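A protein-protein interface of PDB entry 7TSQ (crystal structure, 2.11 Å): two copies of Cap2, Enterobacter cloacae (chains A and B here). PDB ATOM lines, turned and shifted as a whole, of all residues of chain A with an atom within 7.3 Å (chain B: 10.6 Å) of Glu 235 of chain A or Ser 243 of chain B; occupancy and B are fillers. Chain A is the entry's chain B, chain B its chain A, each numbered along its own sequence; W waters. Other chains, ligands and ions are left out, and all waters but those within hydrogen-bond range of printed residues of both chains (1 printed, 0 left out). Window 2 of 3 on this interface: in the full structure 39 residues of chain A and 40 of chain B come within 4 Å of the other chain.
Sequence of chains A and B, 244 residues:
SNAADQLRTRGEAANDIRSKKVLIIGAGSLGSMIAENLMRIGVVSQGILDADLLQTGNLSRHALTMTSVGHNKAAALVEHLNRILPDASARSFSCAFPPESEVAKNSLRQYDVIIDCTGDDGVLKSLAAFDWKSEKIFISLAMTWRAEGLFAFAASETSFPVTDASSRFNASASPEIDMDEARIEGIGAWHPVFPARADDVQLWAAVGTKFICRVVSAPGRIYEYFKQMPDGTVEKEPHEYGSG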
ATOM      1  N   TRP A 204       7.519  29.192  19.988  1.00  0.00           N
ATOM      2  CA  TRP A 204       7.864  28.212  21.009  1.00  0.00           C
ATOM      3  C   TRP A 204       6.684  27.897  21.913  1.00  0.00           C
ATOM      4  O   TRP A 204       6.563  26.763  22.384  1.00  0.00           O
ATOM      5  CB  TRP A 204       9.046  28.707  21.845  1.00  0.00           C
ATOM      6  CG  TRP A 204      10.432  28.605  21.172  1.00  0.00           C
ATOM      7  CD1 TRP A 204      11.458  29.498  21.294  1.00  0.00           C
ATOM      8  CD2 TRP A 204      10.919  27.563  20.303  1.00  0.00           C
ATOM      9  NE1 TRP A 204      12.549  29.080  20.566  1.00  0.00           N
ATOM     10  CE2 TRP A 204      12.244  27.898  19.947  1.00  0.00           C
ATOM     11  CE3 TRP A 204      10.368  26.384  19.795  1.00  0.00           C
ATOM     12  CZ2 TRP A 204      13.020  27.095  19.110  1.00  0.00           C
ATOM     13  CZ3 TRP A 204      11.133  25.593  18.965  1.00  0.00           C
ATOM     14  CH2 TRP A 204      12.446  25.948  18.630  1.00  0.00           C
ATOM     15  N   TYR A 225      15.158  18.899  22.658  1.00  0.00           N
ATOM     16  CA  TYR A 225      15.671  20.250  22.445  1.00  0.00           C
ATOM     17  C   TYR A 225      15.387  20.666  21.006  1.00  0.00           C
ATOM     18  O   TYR A 225      15.876  20.028  20.068  1.00  0.00           O
ATOM     19  CB  TYR A 225      17.177  20.323  22.731  1.00  0.00           C
ATOM     20  CG  TYR A 225      17.787  21.703  22.530  1.00  0.00           C
ATOM     21  CD1 TYR A 225      17.643  22.698  23.492  1.00  0.00           C
ATOM     22  CD2 TYR A 225      18.504  22.014  21.382  1.00  0.00           C
ATOM     23  CE1 TYR A 225      18.187  23.962  23.311  1.00  0.00           C
ATOM     24  CE2 TYR A 225      19.054  23.267  21.193  1.00  0.00           C
ATOM     25  CZ  TYR A 225      18.892  24.241  22.156  1.00  0.00           C
ATOM     26  OH  TYR A 225      19.441  25.493  21.961  1.00  0.00           O
ATOM     27  N   PHE A 226      14.586  21.717  20.837  1.00  0.00           N
ATOM     28  CA  PHE A 226      14.229  22.254  19.530  1.00  0.00           C
ATOM     29  C   PHE A 226      15.108  23.459  19.196  1.00  0.00           C
ATOM     30  O   PHE A 226      15.715  24.081  20.071  1.00  0.00           O
ATOM     31  CB  PHE A 226      12.745  22.654  19.489  1.00  0.00           C
ATOM     32  CG  PHE A 226      11.773  21.490  19.699  1.00  0.00           C
ATOM     33  CD1 PHE A 226      11.364  21.110  20.976  1.00  0.00           C
ATOM     34  CD2 PHE A 226      11.256  20.789  18.615  1.00  0.00           C
ATOM     35  CE1 PHE A 226      10.466  20.054  21.161  1.00  0.00           C
ATOM     36  CE2 PHE A 226      10.364  19.730  18.797  1.00  0.00           C
ATOM     37  CZ  PHE A 226       9.972  19.367  20.069  1.00  0.00           C
ATOM     38  N   LYS A 227      15.198  23.764  17.894  1.00  0.00           N
ATOM     39  CA  LYS A 227      15.972  24.904  17.393  1.00  0.00           C
ATOM     40  C   LYS A 227      15.215  25.597  16.262  1.00  0.00           C
ATOM     41  O   LYS A 227      14.826  24.940  15.289  1.00  0.00           O
ATOM     42  CB  LYS A 227      17.356  24.488  16.866  1.00  0.00           C
ATOM     43  CG  LYS A 227      18.391  23.926  17.854  1.00  0.00           C
ATOM     44  CD  LYS A 227      19.646  23.437  17.091  1.00  0.00           C
ATOM     45  CE  LYS A 227      20.710  22.814  18.004  1.00  0.00           C
ATOM     46  NZ  LYS A 227      21.889  22.263  17.265  1.00  0.00           N
ATOM     47  N   GLN A 228      15.030  26.917  16.364  1.00  0.00           N
ATOM     48  CA  GLN A 228      14.383  27.730  15.332  1.00  0.00           C
ATOM     49  C   GLN A 228      15.412  28.297  14.360  1.00  0.00           C
ATOM     50  O   GLN A 228      16.527  28.643  14.753  1.00  0.00           O
ATOM     51  CB  GLN A 228      13.621  28.846  16.044  1.00  0.00           C
ATOM     52  CG  GLN A 228      13.173  30.045  15.259  1.00  0.00           C
ATOM     53  CD  GLN A 228      12.663  31.156  16.191  1.00  0.00           C
ATOM     54  OE1 GLN A 228      11.507  31.158  16.614  1.00  0.00           O
ATOM     55  NE2 GLN A 228      13.547  32.085  16.535  1.00  0.00           N
ATOM     56  N   MET A 229      15.063  28.308  13.076  1.00  0.00           N
ATOM     57  CA  MET A 229      15.887  28.877  12.016  1.00  0.00           C
ATOM     58  C   MET A 229      15.374  30.258  11.645  1.00  0.00           C
ATOM     59  O   MET A 229      14.320  30.691  12.122  1.00  0.00           O
ATOM     60  CB  MET A 229      15.866  27.964  10.789  1.00  0.00           C
ATOM     61  CG  MET A 229      16.194  26.506  11.066  1.00  0.00           C
ATOM     62  SD  MET A 229      17.884  26.159  11.605  1.00  0.00           S
ATOM     63  CE  MET A 229      17.579  25.246  13.111  1.00  0.00           C
ATOM     64  N   GLY A 232      11.702  30.473  10.423  1.00  0.00           N
ATOM     65  CA  GLY A 232      10.669  29.884  11.240  1.00  0.00           C
ATOM     66  C   GLY A 232      10.582  28.375  11.214  1.00  0.00           C
ATOM     67  O   GLY A 232       9.741  27.819  11.929  1.00  0.00           O
ATOM     68  N   THR A 233      11.366  27.694  10.379  1.00  0.00           N
ATOM     69  CA  THR A 233      11.405  26.237  10.426  1.00  0.00           C
ATOM     70  C   THR A 233      12.043  25.783  11.738  1.00  0.00           C
ATOM     71  O   THR A 233      12.815  26.519  12.361  1.00  0.00           O
ATOM     72  CB  THR A 233      12.179  25.673   9.235  1.00  0.00           C
ATOM     73  OG1 THR A 233      13.509  26.203   9.196  1.00  0.00           O
ATOM     74  CG2 THR A 233      11.454  26.034   7.929  1.00  0.00           C
ATOM     75  N   VAL A 234      11.669  24.579  12.187  1.00  0.00           N
ATOM     76  CA  VAL A 234      12.090  24.044  13.484  1.00  0.00           C
ATOM     77  C   VAL A 234      12.710  22.667  13.296  1.00  0.00           C
ATOM     78  O   VAL A 234      12.190  21.846  12.533  1.00  0.00           O
ATOM     79  CB  VAL A 234      10.902  23.958  14.474  1.00  0.00           C
ATOM     80  CG1 VAL A 234      11.363  23.402  15.816  1.00  0.00           C
ATOM     81  CG2 VAL A 234      10.234  25.303  14.649  1.00  0.00           C
ATOM     82  N   GLU A 235      13.835  22.422  13.983  1.00  0.00           N
ATOM     83  CA  GLU A 235      14.511  21.127  14.013  1.00  0.00           C
ATOM     84  C   GLU A 235      14.498  20.592  15.444  1.00  0.00           C
ATOM     85  O   GLU A 235      14.336  21.353  16.404  1.00  0.00           O
ATOM     86  CB  GLU A 235      15.961  21.238  13.499  1.00  0.00           C
ATOM     87  CG  GLU A 235      16.074  21.594  11.999  1.00  0.00           C
ATOM     88  CD  GLU A 235      17.503  21.523  11.436  1.00  0.00           C
ATOM     89  OE1 GLU A 235      18.464  21.823  12.173  1.00  0.00           O
ATOM     90  OE2 GLU A 235      17.660  21.163  10.244  1.00  0.00           O
ATOM     91  N   LYS A 236      14.647  19.264  15.594  1.00  0.00           N
ATOM     92  CA  LYS A 236      14.533  18.617  16.900  1.00  0.00           C
ATOM     93  C   LYS A 236      15.647  17.595  17.104  1.00  0.00           C
ATOM     94  O   LYS A 236      16.097  16.942  16.156  1.00  0.00           O
ATOM     95  CB  LYS A 236      13.170  17.897  17.084  1.00  0.00           C
ATOM     96  CG  LYS A 236      12.945  17.278  18.473  1.00  0.00           C
ATOM     97  CD  LYS A 236      11.620  16.507  18.606  1.00  0.00           C
ATOM     98  CE  LYS A 236      11.583  15.253  17.728  1.00  0.00           C
ATOM     99  NZ  LYS A 236      10.673  14.197  18.266  1.00  0.00           N
ATOM    100  N   GLU A 237      16.070  17.441  18.362  1.00  0.00           N
ATOM    101  CA  GLU A 237      17.049  16.423  18.763  1.00  0.00           C
ATOM    102  C   GLU A 237      16.627  15.816  20.085  1.00  0.00           C
ATOM    103  O   GLU A 237      16.921  16.370  21.169  1.00  0.00           O
ATOM    104  CB  GLU A 237      18.461  17.008  18.874  1.00  0.00           C
ATOM    105  CG  GLU A 237      19.054  17.531  17.547  1.00  0.00           C
ATOM    106  CD  GLU A 237      20.422  18.213  17.694  1.00  0.00           C
ATOM    107  OE1 GLU A 237      20.857  18.473  18.836  1.00  0.00           O
ATOM    108  OE2 GLU A 237      21.063  18.495  16.653  1.00  0.00           O
ATOM    109  N   LEU B 203       1.103  28.705  15.611  1.00  0.00           N
ATOM    110  CA  LEU B 203       2.347  28.315  14.971  1.00  0.00           C
ATOM    111  C   LEU B 203       2.465  28.950  13.598  1.00  0.00           C
ATOM    112  O   LEU B 203       3.517  29.485  13.235  1.00  0.00           O
ATOM    113  CB  LEU B 203       2.445  26.795  14.848  1.00  0.00           C
ATOM    114  CG  LEU B 203       3.811  26.214  14.444  1.00  0.00           C
ATOM    115  CD1 LEU B 203       4.747  26.087  15.647  1.00  0.00           C
ATOM    116  CD2 LEU B 203       3.645  24.874  13.744  1.00  0.00           C
ATOM    117  N   VAL B 207       5.048  31.807  12.010  1.00  0.00           N
ATOM    118  CA  VAL B 207       5.820  31.583  10.794  1.00  0.00           C
ATOM    119  C   VAL B 207       5.491  32.616   9.729  1.00  0.00           C
ATOM    120  O   VAL B 207       6.359  33.028   8.950  1.00  0.00           O
ATOM    121  CB  VAL B 207       5.583  30.154  10.276  1.00  0.00           C
ATOM    122  CG1 VAL B 207       6.206  29.975   8.900  1.00  0.00           C
ATOM    123  CG2 VAL B 207       6.154  29.133  11.261  1.00  0.00           C
ATOM    124  N   LYS B 227       5.323  23.152   6.372  1.00  0.00           N
ATOM    125  CA  LYS B 227       4.663  21.902   6.759  1.00  0.00           C
ATOM    126  C   LYS B 227       4.919  21.572   8.231  1.00  0.00           C
ATOM    127  O   LYS B 227       6.072  21.522   8.659  1.00  0.00           O
ATOM    128  CB  LYS B 227       5.142  20.715   5.911  1.00  0.00           C
ATOM    129  CG  LYS B 227       4.773  20.655   4.420  1.00  0.00           C
ATOM    130  CD  LYS B 227       5.374  19.392   3.752  1.00  0.00           C
ATOM    131  CE  LYS B 227       4.914  19.181   2.301  1.00  0.00           C
ATOM    132  NZ  LYS B 227       5.495  17.956   1.662  1.00  0.00           N
ATOM    133  N   MET B 229       5.023  18.805  11.169  1.00  0.00           N
ATOM    134  CA  MET B 229       5.306  17.378  11.251  1.00  0.00           C
ATOM    135  C   MET B 229       4.876  16.815  12.600  1.00  0.00           C
ATOM    136  O   MET B 229       4.785  17.551  13.588  1.00  0.00           O
ATOM    137  CB  MET B 229       6.802  17.099  11.055  1.00  0.00           C
ATOM    138  CG  MET B 229       7.409  17.700   9.796  1.00  0.00           C
ATOM    139  SD  MET B 229       6.726  17.070   8.243  1.00  0.00           S
ATOM    140  CE  MET B 229       7.060  15.315   8.398  1.00  0.00           C
ATOM    141  N   ASP B 231       6.367  15.122  14.837  1.00  0.00           N
ATOM    142  CA  ASP B 231       7.362  15.215  15.897  1.00  0.00           C
ATOM    143  C   ASP B 231       7.588  16.639  16.385  1.00  0.00           C
ATOM    144  O   ASP B 231       8.446  16.845  17.251  1.00  0.00           O
ATOM    145  CB  ASP B 231       8.692  14.597  15.440  1.00  0.00           C
ATOM    146  CG  ASP B 231       9.323  15.330  14.252  1.00  0.00           C
ATOM    147  OD1 ASP B 231       8.598  15.998  13.483  1.00  0.00           O
ATOM    148  OD2 ASP B 231      10.561  15.217  14.085  1.00  0.00           O
ATOM    149  N   GLY B 232       6.823  17.605  15.893  1.00  0.00           N
ATOM    150  CA  GLY B 232       6.925  18.967  16.366  1.00  0.00           C
ATOM    151  C   GLY B 232       7.800  19.886  15.541  1.00  0.00           C
ATOM    152  O   GLY B 232       7.971  21.052  15.921  1.00  0.00           O
ATOM    153  N   THR B 233       8.390  19.390  14.461  1.00  0.00           N
ATOM    154  CA  THR B 233       9.270  20.154  13.590  1.00  0.00           C
ATOM    155  C   THR B 233       8.483  20.796  12.444  1.00  0.00           C
ATOM    156  O   THR B 233       7.363  20.391  12.126  1.00  0.00           O
ATOM    157  CB  THR B 233      10.352  19.237  13.029  1.00  0.00           C
ATOM    158  OG1 THR B 233       9.744  18.188  12.260  1.00  0.00           O
ATOM    159  CG2 THR B 233      11.151  18.597  14.169  1.00  0.00           C
ATOM    160  N   VAL B 234       9.065  21.847  11.862  1.00  0.00           N
ATOM    161  CA  VAL B 234       8.484  22.579  10.734  1.00  0.00           C
ATOM    162  C   VAL B 234       9.474  22.555   9.578  1.00  0.00           C
ATOM    163  O   VAL B 234      10.670  22.791   9.779  1.00  0.00           O
ATOM    164  CB  VAL B 234       8.141  24.032  11.119  1.00  0.00           C
ATOM    165  CG1 VAL B 234       7.570  24.784   9.923  1.00  0.00           C
ATOM    166  CG2 VAL B 234       7.174  24.065  12.290  1.00  0.00           C
ATOM    167  N   GLU B 235       8.975  22.270   8.369  1.00  0.00           N
ATOM    168  CA  GLU B 235       9.792  22.164   7.161  1.00  0.00           C
ATOM    169  C   GLU B 235       9.276  23.150   6.116  1.00  0.00           C
ATOM    170  O   GLU B 235       8.129  23.593   6.182  1.00  0.00           O
ATOM    171  CB  GLU B 235       9.766  20.728   6.596  1.00  0.00           C
ATOM    172  CG  GLU B 235      10.264  19.652   7.589  1.00  0.00           C
ATOM    173  CD  GLU B 235      10.231  18.214   7.047  1.00  0.00           C
ATOM    174  OE1 GLU B 235       9.794  18.010   5.897  1.00  0.00           O
ATOM    175  OE2 GLU B 235      10.647  17.283   7.782  1.00  0.00           O
ATOM    176  N   LYS B 236      10.139  23.515   5.150  1.00  0.00           N
ATOM    177  CA  LYS B 236       9.797  24.494   4.122  1.00  0.00           C
ATOM    178  C   LYS B 236      10.211  23.994   2.738  1.00  0.00           C
ATOM    179  O   LYS B 236      11.238  23.323   2.583  1.00  0.00           O
ATOM    180  CB  LYS B 236      10.469  25.870   4.381  1.00  0.00           C
ATOM    181  CG  LYS B 236       9.935  27.034   3.541  1.00  0.00           C
ATOM    182  CD  LYS B 236      10.725  28.334   3.766  1.00  0.00           C
ATOM    183  CE  LYS B 236      12.045  28.345   2.996  1.00  0.00           C
ATOM    184  NZ  LYS B 236      12.799  29.622   3.168  1.00  0.00           N
ATOM    185  N   PRO B 238      10.665  25.886  -0.845  1.00  0.00           N
ATOM    186  CA  PRO B 238      12.033  25.349  -0.978  1.00  0.00           C
ATOM    187  C   PRO B 238      12.832  25.228   0.309  1.00  0.00           C
ATOM    188  O   PRO B 238      12.706  26.081   1.167  1.00  0.00           O
ATOM    189  CB  PRO B 238      12.699  26.376  -1.891  1.00  0.00           C
ATOM    190  CG  PRO B 238      12.101  27.704  -1.357  1.00  0.00           C
ATOM    191  CD  PRO B 238      10.677  27.365  -0.879  1.00  0.00           C
ATOM    192  N   HIS B 239      13.640  24.181   0.436  1.00  0.00           N
ATOM    193  CA  HIS B 239      14.503  24.055   1.600  1.00  0.00           C
ATOM    194  C   HIS B 239      15.582  25.127   1.563  1.00  0.00           C
ATOM    195  O   HIS B 239      16.142  25.424   0.504  1.00  0.00           O
ATOM    196  CB  HIS B 239      15.155  22.676   1.646  1.00  0.00           C
ATOM    197  CG  HIS B 239      15.943  22.430   2.897  1.00  0.00           C
ATOM    198  ND1 HIS B 239      15.367  21.962   4.061  1.00  0.00           N
ATOM    199  CD2 HIS B 239      17.259  22.603   3.172  1.00  0.00           C
ATOM    200  CE1 HIS B 239      16.295  21.850   4.995  1.00  0.00           C
ATOM    201  NE2 HIS B 239      17.451  22.231   4.483  1.00  0.00           N
ATOM    202  N   GLU B 240      15.859  25.726   2.728  1.00  0.00           N
ATOM    203  CA  GLU B 240      16.918  26.723   2.841  1.00  0.00           C
ATOM    204  C   GLU B 240      17.887  26.425   3.985  1.00  0.00           C
ATOM    205  O   GLU B 240      19.072  26.185   3.740  1.00  0.00           O
ATOM    206  CB  GLU B 240      16.330  28.134   3.011  1.00  0.00           C
ATOM    207  CG  GLU B 240      17.393  29.249   3.063  1.00  0.00           C
ATOM    208  CD  GLU B 240      16.842  30.679   2.957  1.00  0.00           C
ATOM    209  OE1 GLU B 240      15.615  30.861   2.875  1.00  0.00           O
ATOM    210  OE2 GLU B 240      17.661  31.629   2.947  1.00  0.00           O
ATOM    211  N   TYR B 241      17.407  26.424   5.227  1.00  0.00           N
ATOM    212  CA  TYR B 241      18.263  26.285   6.401  1.00  0.00           C
ATOM    213  C   TYR B 241      18.264  24.848   6.925  1.00  0.00           C
ATOM    214  O   TYR B 241      17.258  24.137   6.854  1.00  0.00           O
ATOM    215  CB  TYR B 241      17.811  27.242   7.514  1.00  0.00           C
ATOM    216  CG  TYR B 241      17.861  28.714   7.129  1.00  0.00           C
ATOM    217  CD1 TYR B 241      19.040  29.439   7.233  1.00  0.00           C
ATOM    218  CD2 TYR B 241      16.730  29.379   6.657  1.00  0.00           C
ATOM    219  CE1 TYR B 241      19.102  30.775   6.876  1.00  0.00           C
ATOM    220  CE2 TYR B 241      16.781  30.724   6.300  1.00  0.00           C
ATOM    221  CZ  TYR B 241      17.975  31.414   6.412  1.00  0.00           C
ATOM    222  OH  TYR B 241      18.045  32.746   6.064  1.00  0.00           O
ATOM    223  N   GLY B 242      19.415  24.420   7.451  1.00  0.00           N
ATOM    224  CA  GLY B 242      19.530  23.109   8.071  1.00  0.00           C
ATOM    225  C   GLY B 242      19.977  22.015   7.123  1.00  0.00           C
ATOM    226  O   GLY B 242      20.442  22.256   6.006  1.00  0.00           O
ATOM    227  N   SER B 243      19.826  20.773   7.591  1.00  0.00           N
ATOM    228  CA  SER B 243      20.167  19.605   6.775  1.00  0.00           C
ATOM    229  C   SER B 243      19.058  19.287   5.779  1.00  0.00           C
ATOM    230  O   SER B 243      17.988  18.806   6.164  1.00  0.00           O
ATOM    231  CB  SER B 243      20.425  18.368   7.637  1.00  0.00           C
ATOM    232  OG  SER B 243      20.973  18.693   8.898  1.00  0.00           O
HETATM  233  O   HOH W   1      14.822  24.084   8.008  1.00  0.00           O
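Glu 235 of chain A touches just these residues of chain B: Gly 242 and Ser 243. Of the printed residues of chain A, Ser 243 of chain B touches Glu 235. Of the printed residues of chain B, Phe 226 of chain A touches Asp 231 (3.8 Å) and Gly 232 (3.97 Å). No residue of chain B comes within 4 Å of Lys 227 of chain A. Val 234 of chain A touches just these residues of chain B: Thr 233 and Val 234. Of the printed residues of chain A, Thr 233 of chain B touches Val 234 (3.2 Å) and Lys 236 (3.6 Å). Printed residues of chain A within 4 Å of Val 207 of chain B: Gly 232. Of the printed residues of chain B, Thr 233 of chain A touches Val 234 (3.3 Å) and Lys 236 (3.7 Å). His 239 of chain B touches none of the printed residues of chain A. The nearest residue of chain B that does not touch Glu 235 of chain A is Thr 233 of chain B (4.1 Å). The nearest printed residue of chain A that does not touch Val 234 of chain B is Gly 232 of chain A (4.2 Å).
Phe 226 of chain A touches Asp 231 of chain B (CE2 to O, 3.8 Å). Gly 232 of chain B touches Phe 226 of chain A (O to CE2, 3.97 Å). CB of Tyr 241 of chain B touches CB of Met 229 of chain A (3.9 Å). Val 207 of chain B touches Gly 232 of chain A (CG2 to O, 3.9 Å). Thr 233 of chain A touches Val 234 of chain B. Thr 233 of chain A touches Lys 236 of chain B (CG2 to CB, 3.7 Å). Val 234 of chain A touches Thr 233 of chain B. OE2 of Glu 235 of chain A touches CA of Gly 242 of chain B, 3.5 Å away. Lys 236 of chain A touches Asp 231 of chain B. CG2 of Thr 233 of chain B touches CB of Lys 236 of chain A, 3.6 Å away.
The backbone carbonyl oxygen (O) of Val 234 of chain B lies within hydrogen-bond range of the backbone NH (N) of Val 234 of chain A, 3.2 Å away. The side-chain carboxylate (OE2) of Glu 235 of chain A sits at hydrogen-bond distance from the backbone NH (N) of Ser 243 of chain B (3.4 Å).
Thr 233 of chain A touches Val 234 of chain B, and with the chains exchanged Val 234 of chain A touches Thr 233 of chain B. Thr 233 of chain A touches Lys 236 of chain B, and with the chains exchanged Lys 236 of chain A touches Thr 233 of chain B. Val 234 of chain B touches its own counterpart, Val 234 of chain A. Positions printed for both chains: 227, 229, 232, 233, 234, 235 and 236.
Hydrophobic or aromatic side chains of chain A that line the printed part of chain B: Phe 226, Met 229 and Val 234. Printed residues of chain B that touch a printed residue of chain A: Val 207, Asp 231, Gly 232, Thr 233, Val 234, Lys 236, Tyr 241, Gly 242 and Ser 243. Hydrophobic or aromatic side chains of chain B that line the printed part of chain A: Val 207, Val 234 and Tyr 241. Among the printed residues, 12 pairs touch across the chains. Among the printed residues, no Asp or Glu carboxylate lies within 4 Å of a Lys or Arg side-chain nitrogen of the other chain.
A ring nitrogen (NE2) of His 239 of chain B lies within hydrogen-bond range of the backbone carbonyl oxygen of Gly 242 of chain B (3.4 Å). A ring nitrogen (NE2) of His 239 of chain B sits at hydrogen-bond distance from the backbone carbonyl oxygen (O) of Tyr 241 of chain B, at 3.0 Å. NZ of Lys 236 of chain B is in salt-bridge range of OE1 of Glu 240 of chain B, 3.1 Å away. N of Lys 227 of chain A is in hydrogen-bond range of O of Glu 235 of chain A (3.0 Å). OE2 of Glu 240 of chain B lies within hydrogen-bond range of OH of Tyr 241 of chain B. The side-chain carboxylate of Asp 231 of chain B lies within hydrogen-bond range of the side-chain hydroxyl of Thr 233 of chain B (2.8 Å).
Water W1 lies within hydrogen-bond range of the backbone carbonyl oxygen (O) of Tyr 241 of chain B (2.7 Å) and the side-chain hydroxyl (OG1) of Thr 233 of chain A (2.8 Å).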
